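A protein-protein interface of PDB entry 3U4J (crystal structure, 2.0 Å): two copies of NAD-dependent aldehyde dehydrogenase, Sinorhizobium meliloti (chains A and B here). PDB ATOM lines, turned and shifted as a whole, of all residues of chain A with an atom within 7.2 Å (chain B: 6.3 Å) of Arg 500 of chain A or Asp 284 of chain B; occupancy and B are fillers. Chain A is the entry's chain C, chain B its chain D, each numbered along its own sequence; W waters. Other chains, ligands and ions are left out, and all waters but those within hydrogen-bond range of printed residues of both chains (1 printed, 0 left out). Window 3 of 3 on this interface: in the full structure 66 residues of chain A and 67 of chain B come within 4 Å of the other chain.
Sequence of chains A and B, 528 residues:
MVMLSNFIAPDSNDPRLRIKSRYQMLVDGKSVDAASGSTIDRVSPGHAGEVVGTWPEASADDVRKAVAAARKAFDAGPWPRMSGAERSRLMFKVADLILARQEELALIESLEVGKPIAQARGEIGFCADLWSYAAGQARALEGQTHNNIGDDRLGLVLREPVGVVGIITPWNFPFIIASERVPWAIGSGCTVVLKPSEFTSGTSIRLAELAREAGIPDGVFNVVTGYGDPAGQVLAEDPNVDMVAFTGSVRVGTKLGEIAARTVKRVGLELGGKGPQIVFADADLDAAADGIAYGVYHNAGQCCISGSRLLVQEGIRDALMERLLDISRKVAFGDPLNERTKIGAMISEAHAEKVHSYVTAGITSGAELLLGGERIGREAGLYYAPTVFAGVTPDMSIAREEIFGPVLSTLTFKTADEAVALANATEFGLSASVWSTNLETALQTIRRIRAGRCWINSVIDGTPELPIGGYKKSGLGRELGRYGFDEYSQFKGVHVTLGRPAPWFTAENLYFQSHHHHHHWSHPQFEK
No position is printed for both chains.
Of the 7 pairs that touch across the chains among the printed residues, none has its exchanged pair printed and touching as well.
The backbone NH (N) of Phe 280 of chain B sits at hydrogen-bond distance from the backbone carbonyl oxygen (O) of Trp 435 of chain B, 3.1 Å away.
OD2 of Asp 284 of chain B sits close to N of Asp 286 of chain B.
OD2 of Asp 284 of chain B sits at hydrogen-bond distance from N of Ala 287 of chain B.
N of Ser 436 of chain B sits close to ND2 of Asn 457 of chain B (3.0 Å).
Asp 284 of chain B touches just one residue of chain A: Arg 500 (3.9 Å).
Printed residues of chain A within 4 Å of Trp 435 of chain B: Pro 501.
Printed residues of chain A within 4 Å of Asp 290 of chain B: Pro 503 (3.5 Å).
Of the printed residues of chain B, Gly 499 of chain A touches Asn 457.
Phe 280 of chain B touches none of the printed residues of chain A.
Leu 285 of chain B touches none of the printed residues of chain A.
The nearest residue of chain A that does not touch Asp 284 of chain B is Gly 499 of chain A (5.5 Å).
The nearest printed residue of chain B that does not touch Pro 503 of chain A is Asp 286 of chain B (6.5 Å).
Water W1 bridges O of Gly 499 of chain A and OD1 of Asn 457 of chain B.
O of Thr 497 of chain A sits close to OD1 of Asn 457 of chain B, at 3.3 Å.
Hydrophobic or aromatic side chains of chain B that line the printed part of chain A: Ala 287 and Trp 435.
Printed residues of chain A that touch a printed residue of chain B: Thr 497, Gly 499, Arg 500, Pro 501 and Pro 503.
Among the printed residues, 7 pairs touch across the chains.
Among the printed residues, pairs that only touch across the chains: Gly 499 of chain A with Asn 457 of chain B (3.6 Å), Arg 500 of chain A with Asp 284 of chain B (3.9 Å), Arg 500 of chain A with Ala 287 of chain B (3.6 Å), Pro 501 of chain A with Trp 435 of chain B (3.9 Å), Pro 501 of chain A with Asn 457 of chain B (3.3 Å) and Pro 503 of chain A with Asp 290 of chain B (3.5 Å).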
ATOM      1  N   ASP A 152      19.489  11.586 -11.499  1.00  0.00           N
ATOM      2  CA  ASP A 152      18.422  12.219 -10.736  1.00  0.00           C
ATOM      3  C   ASP A 152      18.612  12.008  -9.233  1.00  0.00           C
ATOM      4  O   ASP A 152      17.844  12.516  -8.423  1.00  0.00           O
ATOM      5  CB  ASP A 152      17.065  11.633 -11.172  1.00  0.00           C
ATOM      6  CG  ASP A 152      17.085  10.085 -11.280  1.00  0.00           C
ATOM      7  OD1 ASP A 152      18.172   9.448 -11.368  1.00  0.00           O
ATOM      8  OD2 ASP A 152      15.987   9.491 -11.315  1.00  0.00           O
ATOM      9  N   THR A 497      16.771  12.120  -3.888  1.00  0.00           N
ATOM     10  CA  THR A 497      16.220  12.388  -5.195  1.00  0.00           C
ATOM     11  C   THR A 497      16.103  13.878  -5.356  1.00  0.00           C
ATOM     12  O   THR A 497      15.504  14.577  -4.523  1.00  0.00           O
ATOM     13  CB  THR A 497      14.850  11.717  -5.407  1.00  0.00           C
ATOM     14  OG1 THR A 497      15.069  10.309  -5.498  1.00  0.00           O
ATOM     15  CG2 THR A 497      14.197  12.171  -6.728  1.00  0.00           C
ATOM     16  N   LEU A 498      16.706  14.339  -6.438  1.00  0.00           N
ATOM     17  CA  LEU A 498      16.652  15.712  -6.831  1.00  0.00           C
ATOM     18  C   LEU A 498      15.547  15.754  -7.871  1.00  0.00           C
ATOM     19  O   LEU A 498      15.672  15.164  -8.972  1.00  0.00           O
ATOM     20  CB  LEU A 498      17.993  16.147  -7.427  1.00  0.00           C
ATOM     21  CG  LEU A 498      19.202  15.972  -6.506  1.00  0.00           C
ATOM     22  CD1 LEU A 498      20.465  16.105  -7.298  1.00  0.00           C
ATOM     23  CD2 LEU A 498      19.195  16.958  -5.338  1.00  0.00           C
ATOM     24  N   GLY A 499      14.457  16.397  -7.493  1.00  0.00           N
ATOM     25  CA  GLY A 499      13.284  16.474  -8.336  1.00  0.00           C
ATOM     26  C   GLY A 499      12.268  15.527  -7.741  1.00  0.00           C
ATOM     27  O   GLY A 499      11.996  15.574  -6.546  1.00  0.00           O
ATOM     28  N   ARG A 500      11.745  14.642  -8.573  1.00  0.00           N
ATOM     29  CA  ARG A 500      10.748  13.694  -8.105  1.00  0.00           C
ATOM     30  C   ARG A 500      11.020  12.285  -8.614  1.00  0.00           C
ATOM     31  O   ARG A 500      11.536  12.107  -9.720  1.00  0.00           O
ATOM     32  CB  ARG A 500       9.318  14.179  -8.450  1.00  0.00           C
ATOM     33  CG  ARG A 500       8.858  14.003  -9.902  1.00  0.00           C
ATOM     34  CD  ARG A 500       7.372  14.427 -10.085  1.00  0.00           C
ATOM     35  NE  ARG A 500       6.732  13.691 -11.185  1.00  0.00           N
ATOM     36  CZ  ARG A 500       5.710  12.828 -11.068  1.00  0.00           C
ATOM     37  NH1 ARG A 500       5.134  12.562  -9.878  1.00  0.00           N
ATOM     38  NH2 ARG A 500       5.252  12.227 -12.168  1.00  0.00           N
ATOM     39  N   PRO A 501      10.675  11.276  -7.799  1.00  0.00           N
ATOM     40  CA  PRO A 501      10.804   9.922  -8.293  1.00  0.00           C
ATOM     41  C   PRO A 501       9.681   9.603  -9.289  1.00  0.00           C
ATOM     42  O   PRO A 501       8.685  10.348  -9.364  1.00  0.00           O
ATOM     43  CB  PRO A 501      10.687   9.069  -7.020  1.00  0.00           C
ATOM     44  CG  PRO A 501       9.883   9.914  -6.045  1.00  0.00           C
ATOM     45  CD  PRO A 501       9.979  11.352  -6.492  1.00  0.00           C
ATOM     46  N   ALA A 502       9.861   8.532 -10.063  1.00  0.00           N
ATOM     47  CA  ALA A 502       8.802   7.984 -10.928  1.00  0.00           C
ATOM     48  C   ALA A 502       7.682   7.521 -10.007  1.00  0.00           C
ATOM     49  O   ALA A 502       7.967   6.922  -8.967  1.00  0.00           O
ATOM     50  CB  ALA A 502       9.331   6.790 -11.743  1.00  0.00           C
ATOM     51  N   PRO A 503       6.417   7.808 -10.369  1.00  0.00           N
ATOM     52  CA  PRO A 503       5.305   7.456  -9.457  1.00  0.00           C
ATOM     53  C   PRO A 503       5.114   5.940  -9.263  1.00  0.00           C
ATOM     54  O   PRO A 503       5.326   5.155 -10.192  1.00  0.00           O
ATOM     55  CB  PRO A 503       4.078   8.102 -10.121  1.00  0.00           C
ATOM     56  CG  PRO A 503       4.475   8.341 -11.570  1.00  0.00           C
ATOM     57  CD  PRO A 503       5.964   8.669 -11.481  1.00  0.00           C
ATOM     58  N   VAL B 279       6.476  15.886   5.298  1.00  0.00           N
ATOM     59  CA  VAL B 279       6.135  16.596   4.077  1.00  0.00           C
ATOM     60  C   VAL B 279       6.000  18.071   4.411  1.00  0.00           C
ATOM     61  O   VAL B 279       5.067  18.483   5.140  1.00  0.00           O
ATOM     62  CB  VAL B 279       4.874  16.019   3.363  1.00  0.00           C
ATOM     63  CG1 VAL B 279       4.638  16.704   2.011  1.00  0.00           C
ATOM     64  CG2 VAL B 279       5.032  14.512   3.164  1.00  0.00           C
ATOM     65  N   PHE B 280       6.946  18.853   3.882  1.00  0.00           N
ATOM     66  CA  PHE B 280       6.905  20.313   3.980  1.00  0.00           C
ATOM     67  C   PHE B 280       5.990  20.945   2.934  1.00  0.00           C
ATOM     68  O   PHE B 280       5.733  20.358   1.884  1.00  0.00           O
ATOM     69  CB  PHE B 280       8.329  20.895   3.896  1.00  0.00           C
ATOM     70  CG  PHE B 280       9.123  20.656   5.133  1.00  0.00           C
ATOM     71  CD1 PHE B 280       9.023  21.523   6.220  1.00  0.00           C
ATOM     72  CD2 PHE B 280       9.931  19.542   5.242  1.00  0.00           C
ATOM     73  CE1 PHE B 280       9.749  21.293   7.385  1.00  0.00           C
ATOM     74  CE2 PHE B 280      10.667  19.305   6.405  1.00  0.00           C
ATOM     75  CZ  PHE B 280      10.583  20.153   7.467  1.00  0.00           C
ATOM     76  N   ASP B 282       6.440  23.257   0.821  1.00  0.00           N
ATOM     77  CA  ASP B 282       7.029  23.545  -0.488  1.00  0.00           C
ATOM     78  C   ASP B 282       7.389  22.249  -1.275  1.00  0.00           C
ATOM     79  O   ASP B 282       8.094  22.308  -2.300  1.00  0.00           O
ATOM     80  CB  ASP B 282       8.265  24.465  -0.310  1.00  0.00           C
ATOM     81  CG  ASP B 282       9.385  23.798   0.504  1.00  0.00           C
ATOM     82  OD1 ASP B 282       9.404  22.542   0.573  1.00  0.00           O
ATOM     83  OD2 ASP B 282      10.243  24.517   1.080  1.00  0.00           O
ATOM     84  N   ALA B 283       6.915  21.080  -0.809  1.00  0.00           N
ATOM     85  CA  ALA B 283       7.192  19.831  -1.530  1.00  0.00           C
ATOM     86  C   ALA B 283       6.444  19.768  -2.865  1.00  0.00           C
ATOM     87  O   ALA B 283       5.502  20.527  -3.088  1.00  0.00           O
ATOM     88  CB  ALA B 283       6.847  18.607  -0.662  1.00  0.00           C
ATOM     89  N   ASP B 284       6.888  18.890  -3.765  1.00  0.00           N
ATOM     90  CA  ASP B 284       6.107  18.516  -4.943  1.00  0.00           C
ATOM     91  C   ASP B 284       4.932  17.676  -4.462  1.00  0.00           C
ATOM     92  O   ASP B 284       5.076  16.514  -4.038  1.00  0.00           O
ATOM     93  CB  ASP B 284       6.938  17.716  -5.943  1.00  0.00           C
ATOM     94  CG  ASP B 284       6.192  17.435  -7.249  1.00  0.00           C
ATOM     95  OD1 ASP B 284       6.722  17.850  -8.290  1.00  0.00           O
ATOM     96  OD2 ASP B 284       5.091  16.793  -7.256  1.00  0.00           O
ATOM     97  N   LEU B 285       3.756  18.268  -4.511  1.00  0.00           N
ATOM     98  CA  LEU B 285       2.652  17.701  -3.777  1.00  0.00           C
ATOM     99  C   LEU B 285       2.214  16.357  -4.353  1.00  0.00           C
ATOM    100  O   LEU B 285       1.918  15.431  -3.600  1.00  0.00           O
ATOM    101  CB  LEU B 285       1.523  18.717  -3.724  1.00  0.00           C
ATOM    102  CG  LEU B 285       0.109  18.292  -3.391  1.00  0.00           C
ATOM    103  CD1 LEU B 285       0.016  17.886  -1.938  1.00  0.00           C
ATOM    104  CD2 LEU B 285      -0.799  19.494  -3.686  1.00  0.00           C
ATOM    105  N   ASP B 286       2.167  16.261  -5.683  1.00  0.00           N
ATOM    106  CA  ASP B 286       1.766  15.016  -6.355  1.00  0.00           C
ATOM    107  C   ASP B 286       2.784  13.898  -6.119  1.00  0.00           C
ATOM    108  O   ASP B 286       2.417  12.752  -5.849  1.00  0.00           O
ATOM    109  CB  ASP B 286       1.594  15.229  -7.857  1.00  0.00           C
ATOM    110  CG  ASP B 286       0.292  15.992  -8.218  1.00  0.00           C
ATOM    111  OD1 ASP B 286       0.199  16.449  -9.374  1.00  0.00           O
ATOM    112  OD2 ASP B 286      -0.629  16.114  -7.367  1.00  0.00           O
ATOM    113  N   ALA B 287       4.065  14.227  -6.236  1.00  0.00           N
ATOM    114  CA  ALA B 287       5.122  13.250  -5.937  1.00  0.00           C
ATOM    115  C   ALA B 287       5.061  12.798  -4.478  1.00  0.00           C
ATOM    116  O   ALA B 287       5.189  11.607  -4.195  1.00  0.00           O
ATOM    117  CB  ALA B 287       6.502  13.818  -6.295  1.00  0.00           C
ATOM    118  N   ALA B 288       4.854  13.737  -3.549  1.00  0.00           N
ATOM    119  CA  ALA B 288       4.795  13.395  -2.127  1.00  0.00           C
ATOM    120  C   ALA B 288       3.585  12.517  -1.769  1.00  0.00           C
ATOM    121  O   ALA B 288       3.711  11.537  -1.055  1.00  0.00           O
ATOM    122  CB  ALA B 288       4.843  14.639  -1.246  1.00  0.00           C
ATOM    123  N   ALA B 289       2.419  12.882  -2.286  1.00  0.00           N
ATOM    124  CA  ALA B 289       1.206  12.081  -2.065  1.00  0.00           C
ATOM    125  C   ALA B 289       1.403  10.638  -2.486  1.00  0.00           C
ATOM    126  O   ALA B 289       1.047   9.718  -1.751  1.00  0.00           O
ATOM    127  CB  ALA B 289       0.006  12.702  -2.821  1.00  0.00           C
ATOM    128  N   ASP B 290       1.947  10.448  -3.686  1.00  0.00           N
ATOM    129  CA  ASP B 290       2.237   9.120  -4.206  1.00  0.00           C
ATOM    130  C   ASP B 290       3.277   8.393  -3.343  1.00  0.00           C
ATOM    131  O   ASP B 290       3.184   7.165  -3.134  1.00  0.00           O
ATOM    132  CB  ASP B 290       2.720   9.232  -5.668  1.00  0.00           C
ATOM    133  CG  ASP B 290       3.199   7.907  -6.239  1.00  0.00           C
ATOM    134  OD1 ASP B 290       4.414   7.574  -6.077  1.00  0.00           O
ATOM    135  OD2 ASP B 290       2.372   7.181  -6.861  1.00  0.00           O
ATOM    136  N   TRP B 435      10.315  15.337   2.366  1.00  0.00           N
ATOM    137  CA  TRP B 435       9.888  15.880   1.096  1.00  0.00           C
ATOM    138  C   TRP B 435       9.903  17.411   1.178  1.00  0.00           C
ATOM    139  O   TRP B 435       9.208  17.989   2.018  1.00  0.00           O
ATOM    140  CB  TRP B 435       8.474  15.380   0.748  1.00  0.00           C
ATOM    141  CG  TRP B 435       8.399  13.881   0.574  1.00  0.00           C
ATOM    142  CD1 TRP B 435       8.363  12.923   1.574  1.00  0.00           C
ATOM    143  CD2 TRP B 435       8.386  13.161  -0.670  1.00  0.00           C
ATOM    144  NE1 TRP B 435       8.323  11.669   1.019  1.00  0.00           N
ATOM    145  CE2 TRP B 435       8.328  11.777  -0.350  1.00  0.00           C
ATOM    146  CE3 TRP B 435       8.426  13.551  -2.020  1.00  0.00           C
ATOM    147  CZ2 TRP B 435       8.302  10.780  -1.333  1.00  0.00           C
ATOM    148  CZ3 TRP B 435       8.396  12.565  -3.001  1.00  0.00           C
ATOM    149  CH2 TRP B 435       8.338  11.189  -2.649  1.00  0.00           C
ATOM    150  N   SER B 436      10.704  18.056   0.319  1.00  0.00           N
ATOM    151  CA  SER B 436      10.835  19.526   0.289  1.00  0.00           C
ATOM    152  C   SER B 436      11.623  19.909  -0.941  1.00  0.00           C
ATOM    153  O   SER B 436      12.491  19.161  -1.350  1.00  0.00           O
ATOM    154  CB  SER B 436      11.557  20.038   1.535  1.00  0.00           C
ATOM    155  OG  SER B 436      11.739  21.436   1.466  1.00  0.00           O
ATOM    156  N   THR B 437      11.320  21.047  -1.555  1.00  0.00           N
ATOM    157  CA  THR B 437      12.161  21.544  -2.669  1.00  0.00           C
ATOM    158  C   THR B 437      13.250  22.516  -2.179  1.00  0.00           C
ATOM    159  O   THR B 437      13.983  23.076  -2.977  1.00  0.00           O
ATOM    160  CB  THR B 437      11.324  22.309  -3.715  1.00  0.00           C
ATOM    161  OG1 THR B 437      10.540  23.295  -3.034  1.00  0.00           O
ATOM    162  CG2 THR B 437      10.407  21.355  -4.489  1.00  0.00           C
ATOM    163  N   ASN B 457      12.861  13.316  -0.897  1.00  0.00           N
ATOM    164  CA  ASN B 457      11.957  13.272  -2.058  1.00  0.00           C
ATOM    165  C   ASN B 457      11.836  11.873  -2.623  1.00  0.00           C
ATOM    166  O   ASN B 457      11.807  11.693  -3.825  1.00  0.00           O
ATOM    167  CB  ASN B 457      12.377  14.265  -3.166  1.00  0.00           C
ATOM    168  CG  ASN B 457      12.369  15.708  -2.685  1.00  0.00           C
ATOM    169  OD1 ASN B 457      13.246  16.516  -3.057  1.00  0.00           O
ATOM    170  ND2 ASN B 457      11.410  16.038  -1.845  1.00  0.00           N
HETATM  171  O   HOH W   1      11.029  17.753  -5.330  1.00  0.00           O
